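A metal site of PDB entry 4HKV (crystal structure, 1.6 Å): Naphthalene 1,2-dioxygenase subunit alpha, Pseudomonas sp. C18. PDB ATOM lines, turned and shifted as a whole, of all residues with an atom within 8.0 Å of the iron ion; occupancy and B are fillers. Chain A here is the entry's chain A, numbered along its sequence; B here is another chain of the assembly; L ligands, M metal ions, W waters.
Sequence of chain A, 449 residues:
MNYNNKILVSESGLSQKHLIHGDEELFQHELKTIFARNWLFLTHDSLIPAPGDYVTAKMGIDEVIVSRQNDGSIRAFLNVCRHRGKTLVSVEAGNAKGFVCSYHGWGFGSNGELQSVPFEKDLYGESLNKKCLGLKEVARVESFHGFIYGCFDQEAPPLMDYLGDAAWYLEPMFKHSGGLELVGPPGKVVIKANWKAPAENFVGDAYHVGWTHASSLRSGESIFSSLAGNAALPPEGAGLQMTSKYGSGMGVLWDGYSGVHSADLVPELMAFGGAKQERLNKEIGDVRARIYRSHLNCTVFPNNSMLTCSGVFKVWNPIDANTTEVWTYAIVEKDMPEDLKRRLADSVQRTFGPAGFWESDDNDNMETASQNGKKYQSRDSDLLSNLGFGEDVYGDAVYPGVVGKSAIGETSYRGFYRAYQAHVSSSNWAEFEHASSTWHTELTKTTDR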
ATOM      1  N   ASN A 201      -4.877  30.100  -9.219  1.00  0.00           N
ATOM      2  CA  ASN A 201      -4.863  29.246  -8.041  1.00  0.00           C
ATOM      3  C   ASN A 201      -4.382  30.034  -6.839  1.00  0.00           C
ATOM      4  O   ASN A 201      -5.005  30.017  -5.780  1.00  0.00           O
ATOM      5  CB  ASN A 201      -3.984  28.013  -8.299  1.00  0.00           C
ATOM      6  CG  ASN A 201      -3.876  27.137  -7.082  1.00  0.00           C
ATOM      7  OD1 ASN A 201      -3.087  27.406  -6.172  1.00  0.00           O
ATOM      8  ND2 ASN A 201      -4.689  26.086  -7.025  1.00  0.00           N
ATOM      9  N   PHE A 202      -3.282  30.769  -7.006  1.00  0.00           N
ATOM     10  CA  PHE A 202      -2.777  31.571  -5.901  1.00  0.00           C
ATOM     11  C   PHE A 202      -3.652  32.765  -5.551  1.00  0.00           C
ATOM     12  O   PHE A 202      -3.672  33.183  -4.395  1.00  0.00           O
ATOM     13  CB  PHE A 202      -1.351  32.054  -6.168  1.00  0.00           C
ATOM     14  CG  PHE A 202      -0.291  31.048  -5.796  1.00  0.00           C
ATOM     15  CD1 PHE A 202      -0.221  29.826  -6.461  1.00  0.00           C
ATOM     16  CD2 PHE A 202       0.618  31.329  -4.797  1.00  0.00           C
ATOM     17  CE1 PHE A 202       0.746  28.898  -6.136  1.00  0.00           C
ATOM     18  CE2 PHE A 202       1.607  30.391  -4.453  1.00  0.00           C
ATOM     19  CZ  PHE A 202       1.654  29.173  -5.125  1.00  0.00           C
ATOM     20  N   ASP A 205      -7.787  30.554  -4.613  1.00  0.00           N
ATOM     21  CA  ASP A 205      -8.243  29.178  -4.437  1.00  0.00           C
ATOM     22  C   ASP A 205      -7.848  28.559  -3.102  1.00  0.00           C
ATOM     23  O   ASP A 205      -6.753  27.999  -2.955  1.00  0.00           O
ATOM     24  CB  ASP A 205      -7.756  28.294  -5.588  1.00  0.00           C
ATOM     25  CG  ASP A 205      -8.592  27.047  -5.749  1.00  0.00           C
ATOM     26  OD1 ASP A 205      -8.883  26.381  -4.722  1.00  0.00           O
ATOM     27  OD2 ASP A 205      -8.976  26.745  -6.896  1.00  0.00           O
ATOM     28  N   HIS A 208      -9.264  24.216  -2.969  1.00  0.00           N
ATOM     29  CA  HIS A 208      -8.469  23.039  -3.359  1.00  0.00           C
ATOM     30  C   HIS A 208      -7.551  22.482  -2.273  1.00  0.00           C
ATOM     31  O   HIS A 208      -7.099  21.341  -2.360  1.00  0.00           O
ATOM     32  CB  HIS A 208      -7.622  23.343  -4.614  1.00  0.00           C
ATOM     33  CG  HIS A 208      -6.304  23.989  -4.328  1.00  0.00           C
ATOM     34  ND1 HIS A 208      -6.191  25.285  -3.870  1.00  0.00           N
ATOM     35  CD2 HIS A 208      -5.036  23.522  -4.435  1.00  0.00           C
ATOM     36  CE1 HIS A 208      -4.907  25.587  -3.706  1.00  0.00           C
ATOM     37  NE2 HIS A 208      -4.191  24.529  -4.050  1.00  0.00           N
ATOM     38  N   VAL A 209      -7.261  23.287  -1.258  1.00  0.00           N
ATOM     39  CA  VAL A 209      -6.170  22.977  -0.334  1.00  0.00           C
ATOM     40  C   VAL A 209      -6.332  21.631   0.369  1.00  0.00           C
ATOM     41  O   VAL A 209      -5.434  20.781   0.341  1.00  0.00           O
ATOM     42  CB  VAL A 209      -5.950  24.108   0.688  1.00  0.00           C
ATOM     43  CG1 VAL A 209      -4.921  23.701   1.735  1.00  0.00           C
ATOM     44  CG2 VAL A 209      -5.486  25.358  -0.030  1.00  0.00           C
ATOM     45  N   THR A 212      -6.409  18.669  -2.785  1.00  0.00           N
ATOM     46  CA  THR A 212      -5.159  18.618  -3.542  1.00  0.00           C
ATOM     47  C   THR A 212      -3.959  18.342  -2.655  1.00  0.00           C
ATOM     48  O   THR A 212      -3.084  17.527  -3.001  1.00  0.00           O
ATOM     49  CB  THR A 212      -4.916  19.958  -4.295  1.00  0.00           C
ATOM     50  OG1 THR A 212      -5.830  20.073  -5.386  1.00  0.00           O
ATOM     51  CG2 THR A 212      -3.484  20.018  -4.838  1.00  0.00           C
ATOM     52  N   HIS A 213      -3.902  19.014  -1.505  1.00  0.00           N
ATOM     53  CA  HIS A 213      -2.721  18.948  -0.657  1.00  0.00           C
ATOM     54  C   HIS A 213      -2.915  18.023   0.537  1.00  0.00           C
ATOM     55  O   HIS A 213      -2.188  18.151   1.515  1.00  0.00           O
ATOM     56  CB  HIS A 213      -2.302  20.343  -0.182  1.00  0.00           C
ATOM     57  CG  HIS A 213      -1.904  21.263  -1.295  1.00  0.00           C
ATOM     58  ND1 HIS A 213      -0.763  21.068  -2.051  1.00  0.00           N
ATOM     59  CD2 HIS A 213      -2.495  22.379  -1.787  1.00  0.00           C
ATOM     60  CE1 HIS A 213      -0.670  22.033  -2.960  1.00  0.00           C
ATOM     61  NE2 HIS A 213      -1.711  22.825  -2.821  1.00  0.00           N
ATOM     62  N   LEU A 307       2.653  33.773  -1.012  1.00  0.00           N
ATOM     63  CA  LEU A 307       1.993  33.394   0.237  1.00  0.00           C
ATOM     64  C   LEU A 307       2.774  34.119   1.320  1.00  0.00           C
ATOM     65  O   LEU A 307       3.912  33.748   1.609  1.00  0.00           O
ATOM     66  CB  LEU A 307       2.116  31.885   0.486  1.00  0.00           C
ATOM     67  CG  LEU A 307       1.637  30.957  -0.647  1.00  0.00           C
ATOM     68  CD1 LEU A 307       1.796  29.479  -0.260  1.00  0.00           C
ATOM     69  CD2 LEU A 307       0.202  31.248  -1.023  1.00  0.00           C
ATOM     70  N   PHE A 352       7.615  24.577  -1.599  1.00  0.00           N
ATOM     71  CA  PHE A 352       7.138  25.152  -2.862  1.00  0.00           C
ATOM     72  C   PHE A 352       8.185  25.339  -3.944  1.00  0.00           C
ATOM     73  O   PHE A 352       7.890  25.903  -5.002  1.00  0.00           O
ATOM     74  CB  PHE A 352       6.382  26.466  -2.599  1.00  0.00           C
ATOM     75  CG  PHE A 352       4.953  26.258  -2.184  1.00  0.00           C
ATOM     76  CD1 PHE A 352       4.630  26.050  -0.847  1.00  0.00           C
ATOM     77  CD2 PHE A 352       3.933  26.235  -3.125  1.00  0.00           C
ATOM     78  CE1 PHE A 352       3.309  25.835  -0.458  1.00  0.00           C
ATOM     79  CE2 PHE A 352       2.602  26.019  -2.746  1.00  0.00           C
ATOM     80  CZ  PHE A 352       2.300  25.821  -1.403  1.00  0.00           C
ATOM     81  N   TRP A 358       4.605  20.329  -1.574  1.00  0.00           N
ATOM     82  CA  TRP A 358       3.289  20.943  -1.759  1.00  0.00           C
ATOM     83  C   TRP A 358       3.076  21.303  -3.222  1.00  0.00           C
ATOM     84  O   TRP A 358       2.047  20.956  -3.817  1.00  0.00           O
ATOM     85  CB  TRP A 358       3.151  22.212  -0.925  1.00  0.00           C
ATOM     86  CG  TRP A 358       3.027  21.993   0.554  1.00  0.00           C
ATOM     87  CD1 TRP A 358       3.979  21.474   1.396  1.00  0.00           C
ATOM     88  CD2 TRP A 358       1.925  22.367   1.382  1.00  0.00           C
ATOM     89  NE1 TRP A 358       3.514  21.467   2.694  1.00  0.00           N
ATOM     90  CE2 TRP A 358       2.250  22.010   2.705  1.00  0.00           C
ATOM     91  CE3 TRP A 358       0.678  22.959   1.122  1.00  0.00           C
ATOM     92  CZ2 TRP A 358       1.376  22.224   3.780  1.00  0.00           C
ATOM     93  CZ3 TRP A 358      -0.189  23.174   2.190  1.00  0.00           C
ATOM     94  CH2 TRP A 358       0.161  22.813   3.494  1.00  0.00           C
ATOM     95  N   GLU A 359       4.050  21.992  -3.802  1.00  0.00           N
ATOM     96  CA  GLU A 359       3.947  22.476  -5.189  1.00  0.00           C
ATOM     97  C   GLU A 359       3.731  21.305  -6.144  1.00  0.00           C
ATOM     98  O   GLU A 359       2.994  21.426  -7.125  1.00  0.00           O
ATOM     99  CB  GLU A 359       5.197  23.288  -5.578  1.00  0.00           C
ATOM    100  CG  GLU A 359       5.258  23.742  -7.052  1.00  0.00           C
ATOM    101  CD  GLU A 359       4.880  25.211  -7.270  1.00  0.00           C
ATOM    102  OE1 GLU A 359       4.195  25.800  -6.400  1.00  0.00           O
ATOM    103  OE2 GLU A 359       5.269  25.775  -8.327  1.00  0.00           O
ATOM    104  N   SER A 360       4.332  20.162  -5.843  1.00  0.00           N
ATOM    105  CA  SER A 360       4.154  18.986  -6.688  1.00  0.00           C
ATOM    106  C   SER A 360       2.713  18.498  -6.697  1.00  0.00           C
ATOM    107  O   SER A 360       2.248  17.940  -7.710  1.00  0.00           O
ATOM    108  CB  SER A 360       5.106  17.852  -6.273  1.00  0.00           C
ATOM    109  OG  SER A 360       4.656  17.185  -5.105  1.00  0.00           O
ATOM    110  N   ASP A 361       1.965  18.722  -5.607  1.00  0.00           N
ATOM    111  CA  ASP A 361       0.582  18.273  -5.538  1.00  0.00           C
ATOM    112  C   ASP A 361      -0.254  18.985  -6.596  1.00  0.00           C
ATOM    113  O   ASP A 361      -1.284  18.471  -7.046  1.00  0.00           O
ATOM    114  CB  ASP A 361      -0.067  18.592  -4.186  1.00  0.00           C
ATOM    115  CG  ASP A 361       0.616  17.936  -3.004  1.00  0.00           C
ATOM    116  OD1 ASP A 361       1.234  16.858  -3.143  1.00  0.00           O
ATOM    117  OD2 ASP A 361       0.508  18.512  -1.884  1.00  0.00           O
ATOM    118  N   ASP A 362       0.177  20.200  -6.963  1.00  0.00           N
ATOM    119  CA  ASP A 362      -0.602  21.039  -7.871  1.00  0.00           C
ATOM    120  C   ASP A 362      -0.296  20.727  -9.328  1.00  0.00           C
ATOM    121  O   ASP A 362      -1.083  21.095 -10.201  1.00  0.00           O
ATOM    122  CB  ASP A 362      -0.297  22.532  -7.642  1.00  0.00           C
ATOM    123  CG  ASP A 362      -0.838  23.064  -6.327  1.00  0.00           C
ATOM    124  OD1 ASP A 362      -2.077  23.110  -6.150  1.00  0.00           O
ATOM    125  OD2 ASP A 362      -0.029  23.483  -5.480  1.00  0.00           O
ATOM    126  N   ASN A 363       0.827  20.069  -9.611  1.00  0.00           N
ATOM    127  CA  ASN A 363       1.303  19.869 -10.981  1.00  0.00           C
ATOM    128  C   ASN A 363       0.257  19.348 -11.959  1.00  0.00           C
ATOM    129  O   ASN A 363      -0.001  19.968 -12.994  1.00  0.00           O
ATOM    130  CB  ASN A 363       2.486  18.892 -11.042  1.00  0.00           C
ATOM    131  CG  ASN A 363       3.819  19.548 -10.743  1.00  0.00           C
ATOM    132  OD1 ASN A 363       4.851  18.862 -10.673  1.00  0.00           O
ATOM    133  ND2 ASN A 363       3.825  20.862 -10.557  1.00  0.00           N
ATOM    134  N   ASN A 365      -2.949  19.117 -11.668  1.00  0.00           N
ATOM    135  CA  ASN A 365      -4.109  20.021 -11.752  1.00  0.00           C
ATOM    136  C   ASN A 365      -3.860  21.116 -12.781  1.00  0.00           C
ATOM    137  O   ASN A 365      -4.693  21.320 -13.678  1.00  0.00           O
ATOM    138  CB  ASN A 365      -4.403  20.681 -10.388  1.00  0.00           C
ATOM    139  CG  ASN A 365      -4.855  19.681  -9.327  1.00  0.00           C
ATOM    140  OD1 ASN A 365      -5.368  18.607  -9.647  1.00  0.00           O
ATOM    141  ND2 ASN A 365      -4.665  20.039  -8.063  1.00  0.00           N
ATOM    142  N   MET A 366      -2.732  21.802 -12.653  1.00  0.00           N
ATOM    143  CA  MET A 366      -2.424  22.925 -13.539  1.00  0.00           C
ATOM    144  C   MET A 366      -2.183  22.477 -14.957  1.00  0.00           C
ATOM    145  O   MET A 366      -2.681  23.088 -15.920  1.00  0.00           O
ATOM    146  CB  MET A 366      -1.157  23.684 -13.105  1.00  0.00           C
ATOM    147  CG  MET A 366      -0.781  23.603 -11.666  1.00  0.00           C
ATOM    148  SD  MET A 366      -0.918  25.218 -10.935  1.00  0.00           S
ATOM    149  CE  MET A 366      -2.618  25.447 -11.252  1.00  0.00           C
ATOM    150  N   TYR B 103      -8.648  17.905  -7.909  1.00  0.00           N
ATOM    151  CA  TYR B 103      -8.384  19.334  -7.706  1.00  0.00           C
ATOM    152  C   TYR B 103      -9.213  19.829  -6.519  1.00  0.00           C
ATOM    153  O   TYR B 103      -8.650  20.116  -5.457  1.00  0.00           O
ATOM    154  CB  TYR B 103      -8.670  20.111  -9.002  1.00  0.00           C
ATOM    155  CG  TYR B 103      -8.001  21.476  -9.118  1.00  0.00           C
ATOM    156  CD1 TYR B 103      -7.475  22.123  -8.007  1.00  0.00           C
ATOM    157  CD2 TYR B 103      -7.936  22.124 -10.350  1.00  0.00           C
ATOM    158  CE1 TYR B 103      -6.874  23.386  -8.122  1.00  0.00           C
ATOM    159  CE2 TYR B 103      -7.333  23.373 -10.465  1.00  0.00           C
ATOM    160  CZ  TYR B 103      -6.816  23.998  -9.350  1.00  0.00           C
ATOM    161  OH  TYR B 103      -6.223  25.245  -9.474  1.00  0.00           O
HETATM  162  O1  LIG L   1      -1.618  27.909  -2.597  1.00  0.00           O
HETATM  163  C1  LIG L   1      -2.673  28.408  -2.230  1.00  0.00           C
HETATM  164  N1  LIG L   1      -3.574  28.904  -3.083  1.00  0.00           N
HETATM  165  C2  LIG L   1      -2.943  28.483  -0.747  1.00  0.00           C
HETATM  166  C3  LIG L   1      -2.035  27.917   0.133  1.00  0.00           C
HETATM  167  C4  LIG L   1      -4.091  29.109  -0.265  1.00  0.00           C
HETATM  168  C5  LIG L   1      -4.314  29.165   1.111  1.00  0.00           C
HETATM  169  C6  LIG L   1      -3.406  28.600   1.992  1.00  0.00           C
HETATM  170  C7  LIG L   1      -2.258  27.974   1.509  1.00  0.00           C
HETATM  171 FE    FE M   1      -2.063  24.261  -4.213  1.00  0.00          FE
HETATM  172  O   HOH W   1      -1.270  26.119  -4.383  1.00  0.00           O
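OD1 of Asn 201 lies within hydrogen-bond range of N1 of the ligand (3.5 Å).
A nitrogen (N1) of the ligand sits at hydrogen-bond distance from the backbone carbonyl oxygen (O) of Asn 201, 3.2 Å away.
A nitrogen (N1) of the ligand is in hydrogen-bond range of the backbone carbonyl oxygen of Asp 205, at 3.3 Å.
A ring nitrogen (ND1) of His 213 lies within hydrogen-bond range of the side-chain carboxylate (OD2) of Asp 361.
N of His 208 is in hydrogen-bond range of OD1 of Asp 205, 2.8 Å away.
NE2 of His 208 sits close to ND2 of Asn 201 (3.4 Å).
A ring nitrogen (ND1) of His 213 lies close to the backbone carbonyl oxygen (O) of Trp 358 (3.3 Å).
ND2 of Asn 201 lies within hydrogen-bond range of OH of Tyr 103 of chain B, at 3.0 Å.
Residues that only touch the iron ion: Asn 201 (3.8 Å).
Four residues have an atom within 4 Å of the iron ion: Asn 201, His 208, His 213 and Asp 362.
The iron ion is bound by water W1 (2.0 Å), NE2 of His 213 (2.0 Å), NE2 of His 208 (2.2 Å), OD1 of Asp 362 (2.3 Å) and OD2 of Asp 362 (2.5 Å).
Water W1 bridges O1 of the ligand and OD1 of Asn 201.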
